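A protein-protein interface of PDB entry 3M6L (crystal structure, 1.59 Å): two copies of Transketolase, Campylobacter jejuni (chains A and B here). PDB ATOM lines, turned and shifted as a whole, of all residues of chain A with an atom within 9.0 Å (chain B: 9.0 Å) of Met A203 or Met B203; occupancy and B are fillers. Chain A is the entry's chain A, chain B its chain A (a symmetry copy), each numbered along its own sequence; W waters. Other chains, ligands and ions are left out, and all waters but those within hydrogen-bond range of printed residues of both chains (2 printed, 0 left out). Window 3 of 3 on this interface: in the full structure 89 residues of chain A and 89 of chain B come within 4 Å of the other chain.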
ATOM      1  N   ASN A 198     -18.353  13.854  21.970  1.00  0.00           N
ATOM      2  CA  ASN A 198     -18.429  13.730  20.473  1.00  0.00           C
ATOM      3  C   ASN A 198     -17.167  13.210  19.829  1.00  0.00           C
ATOM      4  O   ASN A 198     -16.943  13.479  18.619  1.00  0.00           O
ATOM      5  CB  ASN A 198     -18.892  15.035  19.872  1.00  0.00           C
ATOM      6  CG  ASN A 198     -17.791  16.058  19.807  1.00  0.00           C
ATOM      7  OD1 ASN A 198     -16.773  15.942  20.464  1.00  0.00           O
ATOM      8  ND2 ASN A 198     -17.975  17.087  18.921  1.00  0.00           N
ATOM      9  N   GLU A 199     -16.376  12.379  20.495  1.00  0.00           N
ATOM     10  CA  GLU A 199     -15.194  11.785  19.983  1.00  0.00           C
ATOM     11  C   GLU A 199     -15.517  10.870  18.821  1.00  0.00           C
ATOM     12  O   GLU A 199     -16.651  10.327  18.742  1.00  0.00           O
ATOM     13  CB  GLU A 199     -14.554  10.845  21.016  1.00  0.00           C
ATOM     14  CG  GLU A 199     -14.109  11.529  22.224  1.00  0.00           C
ATOM     15  CD  GLU A 199     -13.385  10.611  23.215  1.00  0.00           C
ATOM     16  OE1 GLU A 199     -13.280   9.402  23.028  1.00  0.00           O
ATOM     17  OE2 GLU A 199     -12.855  11.151  24.217  1.00  0.00           O
ATOM     18  N   ASN A 200     -14.536  10.751  17.953  1.00  0.00           N
ATOM     19  CA  ASN A 200     -14.552   9.703  16.936  1.00  0.00           C
ATOM     20  C   ASN A 200     -14.121   8.406  17.591  1.00  0.00           C
ATOM     21  O   ASN A 200     -12.920   8.122  17.762  1.00  0.00           O
ATOM     22  CB  ASN A 200     -13.685  10.066  15.751  1.00  0.00           C
ATOM     23  CG  ASN A 200     -13.795   9.085  14.597  1.00  0.00           C
ATOM     24  OD1 ASN A 200     -14.062   7.896  14.773  1.00  0.00           O
ATOM     25  ND2 ASN A 200     -13.487   9.581  13.392  1.00  0.00           N
ATOM     26  N   VAL A 201     -15.120   7.610  18.011  1.00  0.00           N
ATOM     27  CA  VAL A 201     -14.805   6.425  18.865  1.00  0.00           C
ATOM     28  C   VAL A 201     -13.963   5.390  18.091  1.00  0.00           C
ATOM     29  O   VAL A 201     -13.092   4.813  18.600  1.00  0.00           O
ATOM     30  CB  VAL A 201     -16.078   5.813  19.462  1.00  0.00           C
ATOM     31  CG1 VAL A 201     -15.684   4.530  20.254  1.00  0.00           C
ATOM     32  CG2 VAL A 201     -16.753   6.823  20.339  1.00  0.00           C
ATOM     33  N   LYS A 202     -14.271   5.160  16.815  1.00  0.00           N
ATOM     34  CA  LYS A 202     -13.508   4.247  16.003  1.00  0.00           C
ATOM     35  C   LYS A 202     -12.084   4.632  15.919  1.00  0.00           C
ATOM     36  O   LYS A 202     -11.157   3.861  16.136  1.00  0.00           O
ATOM     37  CB  LYS A 202     -14.184   4.230  14.600  1.00  0.00           C
ATOM     38  CG  LYS A 202     -13.416   3.401  13.588  1.00  0.00           C
ATOM     39  CD  LYS A 202     -14.297   3.282  12.328  1.00  0.00           C
ATOM     40  CE  LYS A 202     -13.880   2.152  11.419  1.00  0.00           C
ATOM     41  NZ  LYS A 202     -12.654   2.407  10.749  1.00  0.00           N
ATOM     42  N   MET A 203     -11.864   5.931  15.674  1.00  0.00           N
ATOM     43  CA  MET A 203     -10.497   6.436  15.585  1.00  0.00           C
ATOM     44  C   MET A 203      -9.780   6.350  16.909  1.00  0.00           C
ATOM     45  O   MET A 203      -8.616   6.029  16.956  1.00  0.00           O
ATOM     46  CB  MET A 203     -10.408   7.882  15.045  1.00  0.00           C
ATOM     47  CG  MET A 203      -8.973   8.295  14.818  1.00  0.00           C
ATOM     48  SD  MET A 203      -8.832  10.151  14.037  1.00  0.00           S
ATOM     49  CE  MET A 203     -10.629  10.434  13.592  1.00  0.00           C
ATOM     50  N   ARG A 204     -10.465   6.657  17.991  1.00  0.00           N
ATOM     51  CA  ARG A 204      -9.870   6.489  19.301  1.00  0.00           C
ATOM     52  C   ARG A 204      -9.282   5.095  19.527  1.00  0.00           C
ATOM     53  O   ARG A 204      -8.166   4.880  20.006  1.00  0.00           O
ATOM     54  CB  ARG A 204     -10.924   6.848  20.318  1.00  0.00           C
ATOM     55  CG  ARG A 204     -10.663   6.339  21.729  1.00  0.00           C
ATOM     56  CD  ARG A 204     -11.865   6.597  22.608  1.00  0.00           C
ATOM     57  NE  ARG A 204     -11.795   5.865  23.872  1.00  0.00           N
ATOM     58  CZ  ARG A 204     -12.590   6.120  24.903  1.00  0.00           C
ATOM     59  NH1 ARG A 204     -13.529   7.002  24.823  1.00  0.00           N
ATOM     60  NH2 ARG A 204     -12.469   5.335  25.994  1.00  0.00           N
ATOM     61  N   PHE A 205     -10.090   4.062  19.246  1.00  0.00           N
ATOM     62  CA  PHE A 205      -9.749   2.721  19.538  1.00  0.00           C
ATOM     63  C   PHE A 205      -8.746   2.115  18.551  1.00  0.00           C
ATOM     64  O   PHE A 205      -7.889   1.332  18.910  1.00  0.00           O
ATOM     65  CB  PHE A 205     -11.065   1.902  19.614  1.00  0.00           C
ATOM     66  CG  PHE A 205     -11.694   1.927  21.050  1.00  0.00           C
ATOM     67  CD1 PHE A 205     -12.571   2.948  21.372  1.00  0.00           C
ATOM     68  CD2 PHE A 205     -11.375   0.952  21.949  1.00  0.00           C
ATOM     69  CE1 PHE A 205     -13.160   2.994  22.579  1.00  0.00           C
ATOM     70  CE2 PHE A 205     -11.994   0.971  23.194  1.00  0.00           C
ATOM     71  CZ  PHE A 205     -12.838   2.019  23.510  1.00  0.00           C
ATOM     72  N   GLU A 206      -8.828   2.588  17.286  1.00  0.00           N
ATOM     73  CA  GLU A 206      -7.796   2.222  16.348  1.00  0.00           C
ATOM     74  C   GLU A 206      -6.471   2.766  16.734  1.00  0.00           C
ATOM     75  O   GLU A 206      -5.434   2.083  16.630  1.00  0.00           O
ATOM     76  CB  GLU A 206      -8.231   2.555  14.890  1.00  0.00           C
ATOM     77  CG  GLU A 206      -9.444   1.787  14.389  1.00  0.00           C
ATOM     78  CD  GLU A 206      -9.855   2.165  12.989  1.00  0.00           C
ATOM     79  OE1 GLU A 206     -10.754   1.480  12.452  1.00  0.00           O
ATOM     80  OE2 GLU A 206      -9.283   3.156  12.428  1.00  0.00           O
ATOM     81  N   ALA A 207      -6.509   3.956  17.375  1.00  0.00           N
ATOM     82  CA  ALA A 207      -5.234   4.575  17.868  1.00  0.00           C
ATOM     83  C   ALA A 207      -4.602   3.742  18.963  1.00  0.00           C
ATOM     84  O   ALA A 207      -3.423   3.764  19.158  1.00  0.00           O
ATOM     85  CB  ALA A 207      -5.418   6.048  18.333  1.00  0.00           C
ATOM     86  N   GLN A 208      -5.413   2.960  19.669  1.00  0.00           N
ATOM     87  CA  GLN A 208      -4.991   2.073  20.699  1.00  0.00           C
ATOM     88  C   GLN A 208      -4.912   0.604  20.333  1.00  0.00           C
ATOM     89  O   GLN A 208      -4.962  -0.292  21.197  1.00  0.00           O
ATOM     90  CB  GLN A 208      -5.946   2.264  21.926  1.00  0.00           C
ATOM     91  CG  GLN A 208      -5.958   3.583  22.541  1.00  0.00           C
ATOM     92  CD  GLN A 208      -6.830   3.658  23.808  1.00  0.00           C
ATOM     93  OE1 GLN A 208      -8.028   3.340  23.802  1.00  0.00           O
ATOM     94  NE2 GLN A 208      -6.264   4.214  24.854  1.00  0.00           N
ATOM     95  N   GLY A 209      -4.823   0.318  19.024  1.00  0.00           N
ATOM     96  CA  GLY A 209      -4.498  -0.984  18.518  1.00  0.00           C
ATOM     97  C   GLY A 209      -5.688  -1.980  18.454  1.00  0.00           C
ATOM     98  O   GLY A 209      -5.442  -3.136  18.403  1.00  0.00           O
ATOM     99  N   PHE A 210      -6.929  -1.492  18.382  1.00  0.00           N
ATOM    100  CA  PHE A 210      -8.153  -2.357  18.290  1.00  0.00           C
ATOM    101  C   PHE A 210      -8.602  -2.449  16.810  1.00  0.00           C
ATOM    102  O   PHE A 210      -8.379  -1.520  15.958  1.00  0.00           O
ATOM    103  CB  PHE A 210      -9.336  -1.731  18.978  1.00  0.00           C
ATOM    104  CG  PHE A 210      -9.326  -1.909  20.485  1.00  0.00           C
ATOM    105  CD1 PHE A 210      -8.379  -1.336  21.256  1.00  0.00           C
ATOM    106  CD2 PHE A 210     -10.321  -2.638  21.098  1.00  0.00           C
ATOM    107  CE1 PHE A 210      -8.424  -1.490  22.706  1.00  0.00           C
ATOM    108  CE2 PHE A 210     -10.368  -2.793  22.482  1.00  0.00           C
ATOM    109  CZ  PHE A 210      -9.455  -2.185  23.251  1.00  0.00           C
ATOM    110  N   VAL A 212     -12.104  -2.377  14.884  1.00  0.00           N
ATOM    111  CA  VAL A 212     -13.366  -1.811  15.190  1.00  0.00           C
ATOM    112  C   VAL A 212     -14.494  -2.108  14.198  1.00  0.00           C
ATOM    113  O   VAL A 212     -14.391  -1.755  13.017  1.00  0.00           O
ATOM    114  CB  VAL A 212     -13.316  -0.270  15.387  1.00  0.00           C
ATOM    115  CG1 VAL A 212     -14.731   0.344  15.743  1.00  0.00           C
ATOM    116  CG2 VAL A 212     -12.126   0.112  16.371  1.00  0.00           C
ATOM    117  N   SER A 214     -18.826  -1.767  13.426  1.00  0.00           N
ATOM    118  CA  SER A 214     -19.945  -0.943  13.734  1.00  0.00           C
ATOM    119  C   SER A 214     -21.203  -1.579  13.199  1.00  0.00           C
ATOM    120  O   SER A 214     -21.308  -1.850  11.994  1.00  0.00           O
ATOM    121  CB  SER A 214     -19.787   0.437  13.086  1.00  0.00           C
ATOM    122  OG  SER A 214     -18.623   1.079  13.670  1.00  0.00           O
ATOM    123  N   LEU A 238     -13.450  -3.986  19.262  1.00  0.00           N
ATOM    124  CA  LEU A 238     -14.608  -3.167  19.687  1.00  0.00           C
ATOM    125  C   LEU A 238     -15.703  -3.309  18.683  1.00  0.00           C
ATOM    126  O   LEU A 238     -15.506  -3.051  17.471  1.00  0.00           O
ATOM    127  CB  LEU A 238     -14.243  -1.669  19.805  1.00  0.00           C
ATOM    128  CG  LEU A 238     -15.386  -0.664  20.088  1.00  0.00           C
ATOM    129  CD1 LEU A 238     -15.882  -0.931  21.475  1.00  0.00           C
ATOM    130  CD2 LEU A 238     -14.932   0.825  19.834  1.00  0.00           C
ATOM    131  N   ILE A 240     -19.070  -1.475  17.985  1.00  0.00           N
ATOM    132  CA  ILE A 240     -19.903  -0.325  18.307  1.00  0.00           C
ATOM    133  C   ILE A 240     -21.315  -0.635  17.859  1.00  0.00           C
ATOM    134  O   ILE A 240     -21.595  -0.687  16.623  1.00  0.00           O
ATOM    135  CB  ILE A 240     -19.421   1.067  17.651  1.00  0.00           C
ATOM    136  CG1 ILE A 240     -17.958   1.314  17.991  1.00  0.00           C
ATOM    137  CG2 ILE A 240     -20.460   2.214  18.012  1.00  0.00           C
ATOM    138  CD1 ILE A 240     -17.271   2.505  17.214  1.00  0.00           C
ATOM    139  N   ASN B 198       2.342   2.429  23.439  1.00  0.00           N
ATOM    140  CA  ASN B 198       2.604   2.507  21.960  1.00  0.00           C
ATOM    141  C   ASN B 198       1.433   3.005  21.148  1.00  0.00           C
ATOM    142  O   ASN B 198       1.361   2.697  19.928  1.00  0.00           O
ATOM    143  CB  ASN B 198       3.136   1.185  21.462  1.00  0.00           C
ATOM    144  CG  ASN B 198       2.049   0.159  21.293  1.00  0.00           C
ATOM    145  OD1 ASN B 198       0.957   0.292  21.814  1.00  0.00           O
ATOM    146  ND2 ASN B 198       2.340  -0.897  20.468  1.00  0.00           N
ATOM    147  N   GLU B 199       0.567   3.855  21.685  1.00  0.00           N
ATOM    148  CA  GLU B 199      -0.541   4.430  21.011  1.00  0.00           C
ATOM    149  C   GLU B 199      -0.074   5.309  19.870  1.00  0.00           C
ATOM    150  O   GLU B 199       1.061   5.852  19.917  1.00  0.00           O
ATOM    151  CB  GLU B 199      -1.303   5.400  21.927  1.00  0.00           C
ATOM    152  CG  GLU B 199      -1.896   4.753  23.091  1.00  0.00           C
ATOM    153  CD  GLU B 199      -2.736   5.700  23.956  1.00  0.00           C
ATOM    154  OE1 GLU B 199      -2.814   6.903  23.720  1.00  0.00           O
ATOM    155  OE2 GLU B 199      -3.387   5.190  24.900  1.00  0.00           O
ATOM    156  N   ASN B 200      -0.940   5.400  18.884  1.00  0.00           N
ATOM    157  CA  ASN B 200      -0.796   6.415  17.845  1.00  0.00           C
ATOM    158  C   ASN B 200      -1.302   7.731  18.401  1.00  0.00           C
ATOM    159  O   ASN B 200      -2.515   8.018  18.412  1.00  0.00           O
ATOM    160  CB  ASN B 200      -1.509   6.014  16.573  1.00  0.00           C
ATOM    161  CG  ASN B 200      -1.255   6.958  15.412  1.00  0.00           C
ATOM    162  OD1 ASN B 200      -1.010   8.153  15.583  1.00  0.00           O
ATOM    163  ND2 ASN B 200      -1.412   6.425  14.194  1.00  0.00           N
ATOM    164  N   VAL B 201      -0.362   8.542  18.916  1.00  0.00           N
ATOM    165  CA  VAL B 201      -0.778   9.752  19.688  1.00  0.00           C
ATOM    166  C   VAL B 201      -1.516  10.760  18.784  1.00  0.00           C
ATOM    167  O   VAL B 201      -2.441  11.352  19.163  1.00  0.00           O
ATOM    168  CB  VAL B 201       0.412  10.385  20.419  1.00  0.00           C
ATOM    169  CG1 VAL B 201      -0.075  11.691  21.116  1.00  0.00           C
ATOM    170  CG2 VAL B 201       0.971   9.403  21.404  1.00  0.00           C
ATOM    171  N   LYS B 202      -1.051  10.951  17.549  1.00  0.00           N
ATOM    172  CA  LYS B 202      -1.705  11.838  16.621  1.00  0.00           C
ATOM    173  C   LYS B 202      -3.109  11.447  16.373  1.00  0.00           C
ATOM    174  O   LYS B 202      -4.054  12.223  16.448  1.00  0.00           O
ATOM    175  CB  LYS B 202      -0.861  11.812  15.313  1.00  0.00           C
ATOM    176  CG  LYS B 202      -1.496  12.608  14.188  1.00  0.00           C
ATOM    177  CD  LYS B 202      -0.464  12.689  13.044  1.00  0.00           C
ATOM    178  CE  LYS B 202      -0.763  13.790  12.055  1.00  0.00           C
ATOM    179  NZ  LYS B 202      -1.896  13.512  11.247  1.00  0.00           N
ATOM    180  N   MET B 203      -3.299  10.141  16.143  1.00  0.00           N
ATOM    181  CA  MET B 203      -4.645   9.631  15.901  1.00  0.00           C
ATOM    182  C   MET B 203      -5.521   9.756  17.122  1.00  0.00           C
ATOM    183  O   MET B 203      -6.682  10.077  17.013  1.00  0.00           O
ATOM    184  CB  MET B 203      -4.669   8.169  15.399  1.00  0.00           C
ATOM    185  CG  MET B 203      -6.066   7.745  15.008  1.00  0.00           C
ATOM    186  SD  MET B 203      -6.113   5.866  14.273  1.00  0.00           S
ATOM    187  CE  MET B 203      -4.275   5.573  14.064  1.00  0.00           C
ATOM    188  N   ARG B 204      -4.976   9.484  18.289  1.00  0.00           N
ATOM    189  CA  ARG B 204      -5.729   9.692  19.510  1.00  0.00           C
ATOM    190  C   ARG B 204      -6.338  11.091  19.617  1.00  0.00           C
ATOM    191  O   ARG B 204      -7.504  11.318  19.947  1.00  0.00           O
ATOM    192  CB  ARG B 204      -4.810   9.367  20.660  1.00  0.00           C
ATOM    193  CG  ARG B 204      -5.244   9.918  22.011  1.00  0.00           C
ATOM    194  CD  ARG B 204      -4.161   9.691  23.040  1.00  0.00           C
ATOM    195  NE  ARG B 204      -4.385  10.462  24.262  1.00  0.00           N
ATOM    196  CZ  ARG B 204      -3.726  10.240  25.392  1.00  0.00           C
ATOM    197  NH1 ARG B 204      -2.786   9.357  25.456  1.00  0.00           N
ATOM    198  NH2 ARG B 204      -3.980  11.059  26.434  1.00  0.00           N
ATOM    199  N   PHE B 205      -5.500  12.117  19.407  1.00  0.00           N
ATOM    200  CA  PHE B 205      -5.871  13.465  19.612  1.00  0.00           C
ATOM    201  C   PHE B 205      -6.743  14.038  18.490  1.00  0.00           C
ATOM    202  O   PHE B 205      -7.636  14.830  18.715  1.00  0.00           O
ATOM    203  CB  PHE B 205      -4.573  14.288  19.826  1.00  0.00           C
ATOM    204  CG  PHE B 205      -4.128  14.310  21.329  1.00  0.00           C
ATOM    205  CD1 PHE B 205      -3.300  13.301  21.788  1.00  0.00           C
ATOM    206  CD2 PHE B 205      -4.554  15.312  22.151  1.00  0.00           C
ATOM    207  CE1 PHE B 205      -2.865  13.294  23.060  1.00  0.00           C
ATOM    208  CE2 PHE B 205      -4.095  15.332  23.463  1.00  0.00           C
ATOM    209  CZ  PHE B 205      -3.298  14.296  23.913  1.00  0.00           C
ATOM    210  N   GLU B 206      -6.505  13.527  17.260  1.00  0.00           N
ATOM    211  CA  GLU B 206      -7.412  13.861  16.190  1.00  0.00           C
ATOM    212  C   GLU B 206      -8.776  13.326  16.425  1.00  0.00           C
ATOM    213  O   GLU B 206      -9.791  14.004  16.173  1.00  0.00           O
ATOM    214  CB  GLU B 206      -6.800  13.483  14.809  1.00  0.00           C
ATOM    215  CG  GLU B 206      -5.533  14.238  14.439  1.00  0.00           C
ATOM    216  CD  GLU B 206      -4.952  13.817  13.113  1.00  0.00           C
ATOM    217  OE1 GLU B 206      -3.992  14.488  12.671  1.00  0.00           O
ATOM    218  OE2 GLU B 206      -5.452  12.808  12.516  1.00  0.00           O
ATOM    219  N   ALA B 207      -8.820  12.157  17.103  1.00  0.00           N
ATOM    220  CA  ALA B 207     -10.147  11.551  17.452  1.00  0.00           C
ATOM    221  C   ALA B 207     -10.909  12.417  18.435  1.00  0.00           C
ATOM    222  O   ALA B 207     -12.103  12.399  18.482  1.00  0.00           O
ATOM    223  CB  ALA B 207     -10.025  10.094  17.983  1.00  0.00           C
ATOM    224  N   GLN B 208     -10.190  13.222  19.211  1.00  0.00           N
ATOM    225  CA  GLN B 208     -10.736  14.140  20.152  1.00  0.00           C
ATOM    226  C   GLN B 208     -10.766  15.596  19.734  1.00  0.00           C
ATOM    227  O   GLN B 208     -10.821  16.519  20.570  1.00  0.00           O
ATOM    228  CB  GLN B 208      -9.940  13.988  21.494  1.00  0.00           C
ATOM    229  CG  GLN B 208     -10.007  12.689  22.146  1.00  0.00           C
ATOM    230  CD  GLN B 208      -9.300  12.655  23.513  1.00  0.00           C
ATOM    231  OE1 GLN B 208      -8.110  12.976  23.647  1.00  0.00           O
ATOM    232  NE2 GLN B 208      -9.992  12.131  24.498  1.00  0.00           N
ATOM    233  N   GLY B 209     -10.691  15.841  18.416  1.00  0.00           N
ATOM    234  CA  GLY B 209     -10.948  17.127  17.834  1.00  0.00           C
ATOM    235  C   GLY B 209      -9.757  18.122  17.886  1.00  0.00           C
ATOM    236  O   GLY B 209      -9.993  19.276  17.769  1.00  0.00           O
ATOM    237  N   PHE B 210      -8.518  17.635  17.984  1.00  0.00           N
ATOM    238  CA  PHE B 210      -7.290  18.498  18.018  1.00  0.00           C
ATOM    239  C   PHE B 210      -6.660  18.545  16.604  1.00  0.00           C
ATOM    240  O   PHE B 210      -6.778  17.591  15.760  1.00  0.00           O
ATOM    241  CB  PHE B 210      -6.203  17.896  18.867  1.00  0.00           C
ATOM    242  CG  PHE B 210      -6.400  18.122  20.355  1.00  0.00           C
ATOM    243  CD1 PHE B 210      -7.437  17.571  21.020  1.00  0.00           C
ATOM    244  CD2 PHE B 210      -5.487  18.871  21.064  1.00  0.00           C
ATOM    245  CE1 PHE B 210      -7.572  17.770  22.458  1.00  0.00           C
ATOM    246  CE2 PHE B 210      -5.612  19.069  22.438  1.00  0.00           C
ATOM    247  CZ  PHE B 210      -6.615  18.484  23.106  1.00  0.00           C
ATOM    248  N   VAL B 212      -2.947  18.420  15.131  1.00  0.00           N
ATOM    249  CA  VAL B 212      -1.733  17.867  15.608  1.00  0.00           C
ATOM    250  C   VAL B 212      -0.490  18.135  14.755  1.00  0.00           C
ATOM    251  O   VAL B 212      -0.446  17.746  13.583  1.00  0.00           O
ATOM    252  CB  VAL B 212      -1.811  16.333  15.845  1.00  0.00           C
ATOM    253  CG1 VAL B 212      -0.452  15.733  16.393  1.00  0.00           C
ATOM    254  CG2 VAL B 212      -3.115  15.979  16.686  1.00  0.00           C
ATOM    255  N   SER B 214       3.903  17.779  14.539  1.00  0.00           N
ATOM    256  CA  SER B 214       4.974  16.967  15.008  1.00  0.00           C
ATOM    257  C   SER B 214       6.289  17.589  14.614  1.00  0.00           C
ATOM    258  O   SER B 214       6.544  17.822  13.424  1.00  0.00           O
ATOM    259  CB  SER B 214       4.895  15.567  14.389  1.00  0.00           C
ATOM    260  OG  SER B 214       3.666  14.941  14.844  1.00  0.00           O
ATOM    261  N   LEU B 238      -2.152  20.168  19.589  1.00  0.00           N
ATOM    262  CA  LEU B 238      -1.057  19.364  20.180  1.00  0.00           C
ATOM    263  C   LEU B 238       0.155  19.477  19.316  1.00  0.00           C
ATOM    264  O   LEU B 238       0.109  19.181  18.098  1.00  0.00           O
ATOM    265  CB  LEU B 238      -1.437  17.870  20.299  1.00  0.00           C
ATOM    266  CG  LEU B 238      -0.340  16.877  20.753  1.00  0.00           C
ATOM    267  CD1 LEU B 238      -0.019  17.188  22.182  1.00  0.00           C
ATOM    268  CD2 LEU B 238      -0.762  15.380  20.490  1.00  0.00           C
ATOM    269  N   ILE B 240       3.579  17.629  19.099  1.00  0.00           N
ATOM    270  CA  ILE B 240       4.363  16.491  19.558  1.00  0.00           C
ATOM    271  C   ILE B 240       5.821  16.789  19.279  1.00  0.00           C
ATOM    272  O   ILE B 240       6.252  16.804  18.086  1.00  0.00           O
ATOM    273  CB  ILE B 240       3.963  15.079  18.891  1.00  0.00           C
ATOM    274  CG1 ILE B 240       2.469  14.839  19.054  1.00  0.00           C
ATOM    275  CG2 ILE B 240       4.947  13.945  19.413  1.00  0.00           C
ATOM    276  CD1 ILE B 240       1.882  13.623  18.234  1.00  0.00           C
HETATM  277  O   HOH W   1      -1.341   1.600  18.419  1.00  0.00           O
HETATM  278  O   HOH W   2     -14.073  14.535  17.424  1.00  0.00           O
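Glu A199 touches Ala B207 (CA to O, 3.5 Å). Met A203 touches Glu B206. Arg A204 touches Ala B207. C of Glu A206 touches SD of Met B203 (3.97 Å). Ala A207 touches Glu B199. CB of Ala A207 touches N of Arg B204, at 3.5 Å.
Of the 17 printed residues of chain A, 7 touch a printed residue of chain B. Printed residues of chain A that touch a printed residue of chain B: Glu A199, Asn A200, Met A203, Arg A204, Glu A206, Ala A207 and Gln A208. Hydrophobic or aromatic side chains of chain A within 4 Å of the printed part of chain B: Met A203 and Ala A207. Of the 17 printed residues of chain B, 7 touch a printed residue of chain A. Printed residues of chain B that touch a printed residue of chain A: Glu B199, Asn B200, Met B203, Arg B204, Glu B206, Ala B207 and Gln B208. Hydrophobic or aromatic side chains of chain B within 4 Å of the printed part of chain A: Met B203 and Ala B207.
Glu A199 touches Gln B208, and with the chains exchanged Gln A208 touches Glu B199. Asn A200 touches Ala B207, and with the chains exchanged Ala A207 touches Asn B200. Met A203 touches Ala B207, and with the chains exchanged Ala A207 touches Met B203. Arg A204 touches Ala B207, and with the chains exchanged Ala A207 touches Arg B204. Positions printed for both chains: 198, 199, 200, 201, 202, 203, 204, 205, 206, 207, 208, 209, 210, 212, 214, 238 and 240.
Water W2 lies within hydrogen-bond range of O of Ala B207 (3.1 Å) and O of Asn A198 (3.3 Å). Water W1 lies within hydrogen-bond range of O of Ala A207 (3.1 Å) and O of Asn B198 (3.3 Å).
OE2 of Glu A199 is in hydrogen-bond range of NE2 of Gln B208 (3.0 Å). The backbone NH (N) of Asn A200 lies within hydrogen-bond range of the backbone carbonyl oxygen (O) of Ala B207 (3.0 Å). SD of Met A203 is in hydrogen-bond range of N of Ala B207, 3.7 Å away. O of Ala A207 lies within hydrogen-bond range of N of Asn B200. The backbone NH of Ala A207 sits at hydrogen-bond distance from the side-chain sulfur of Met B203 (3.7 Å). NE2 of Gln A208 sits at hydrogen-bond distance from OE2 of Glu B199 (3.0 Å). The backbone carbonyl oxygen (O) of Met B203 lies close to the side-chain sulfur (SD) of Met A203 (3.7 Å).
Of the printed residues of chain B, Met A203 touches Met B203, Glu B206 and Ala B207. Of the printed residues of chain A, Met B203 touches Met A203, Glu A206 and Ala A207. Printed residues of chain B within 4 Å of Gln A208: Glu B199 (3.0 Å). Printed residues of chain A within 4 Å of Arg B204: Ala A207 (3.5 Å). Of the printed residues of chain B, Ala A207 touches Glu B199, Asn B200, Met B203 and Arg B204. Gly B209 touches none of the printed residues of chain A. Val B212 touches none of the printed residues of chain A. The nearest printed residue of chain A that does not touch Met B203 is Arg A204 (5.2 Å).
NH1 of Arg A204 lies within salt-bridge range of OE1 of Glu A199 (3.0 Å). The backbone NH (N) of Lys A202 lies close to the side-chain amide oxygen (OD1) of Asn A200. The backbone NH (N) of Met A203 lies within hydrogen-bond range of the side-chain amide oxygen (OD1) of Asn A200 (3.1 Å). The side-chain carboxylate (OE1) of Glu B199 lies within salt-bridge range of the guanidinium group (NH1) of Arg B204, at 3.0 Å. OD1 of Asn B200 sits at hydrogen-bond distance from N of Met B203 (3.1 Å). The side-chain carboxylate of Glu B206 is in salt-bridge range of the side-chain amino group of Lys B202 (2.7 Å).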
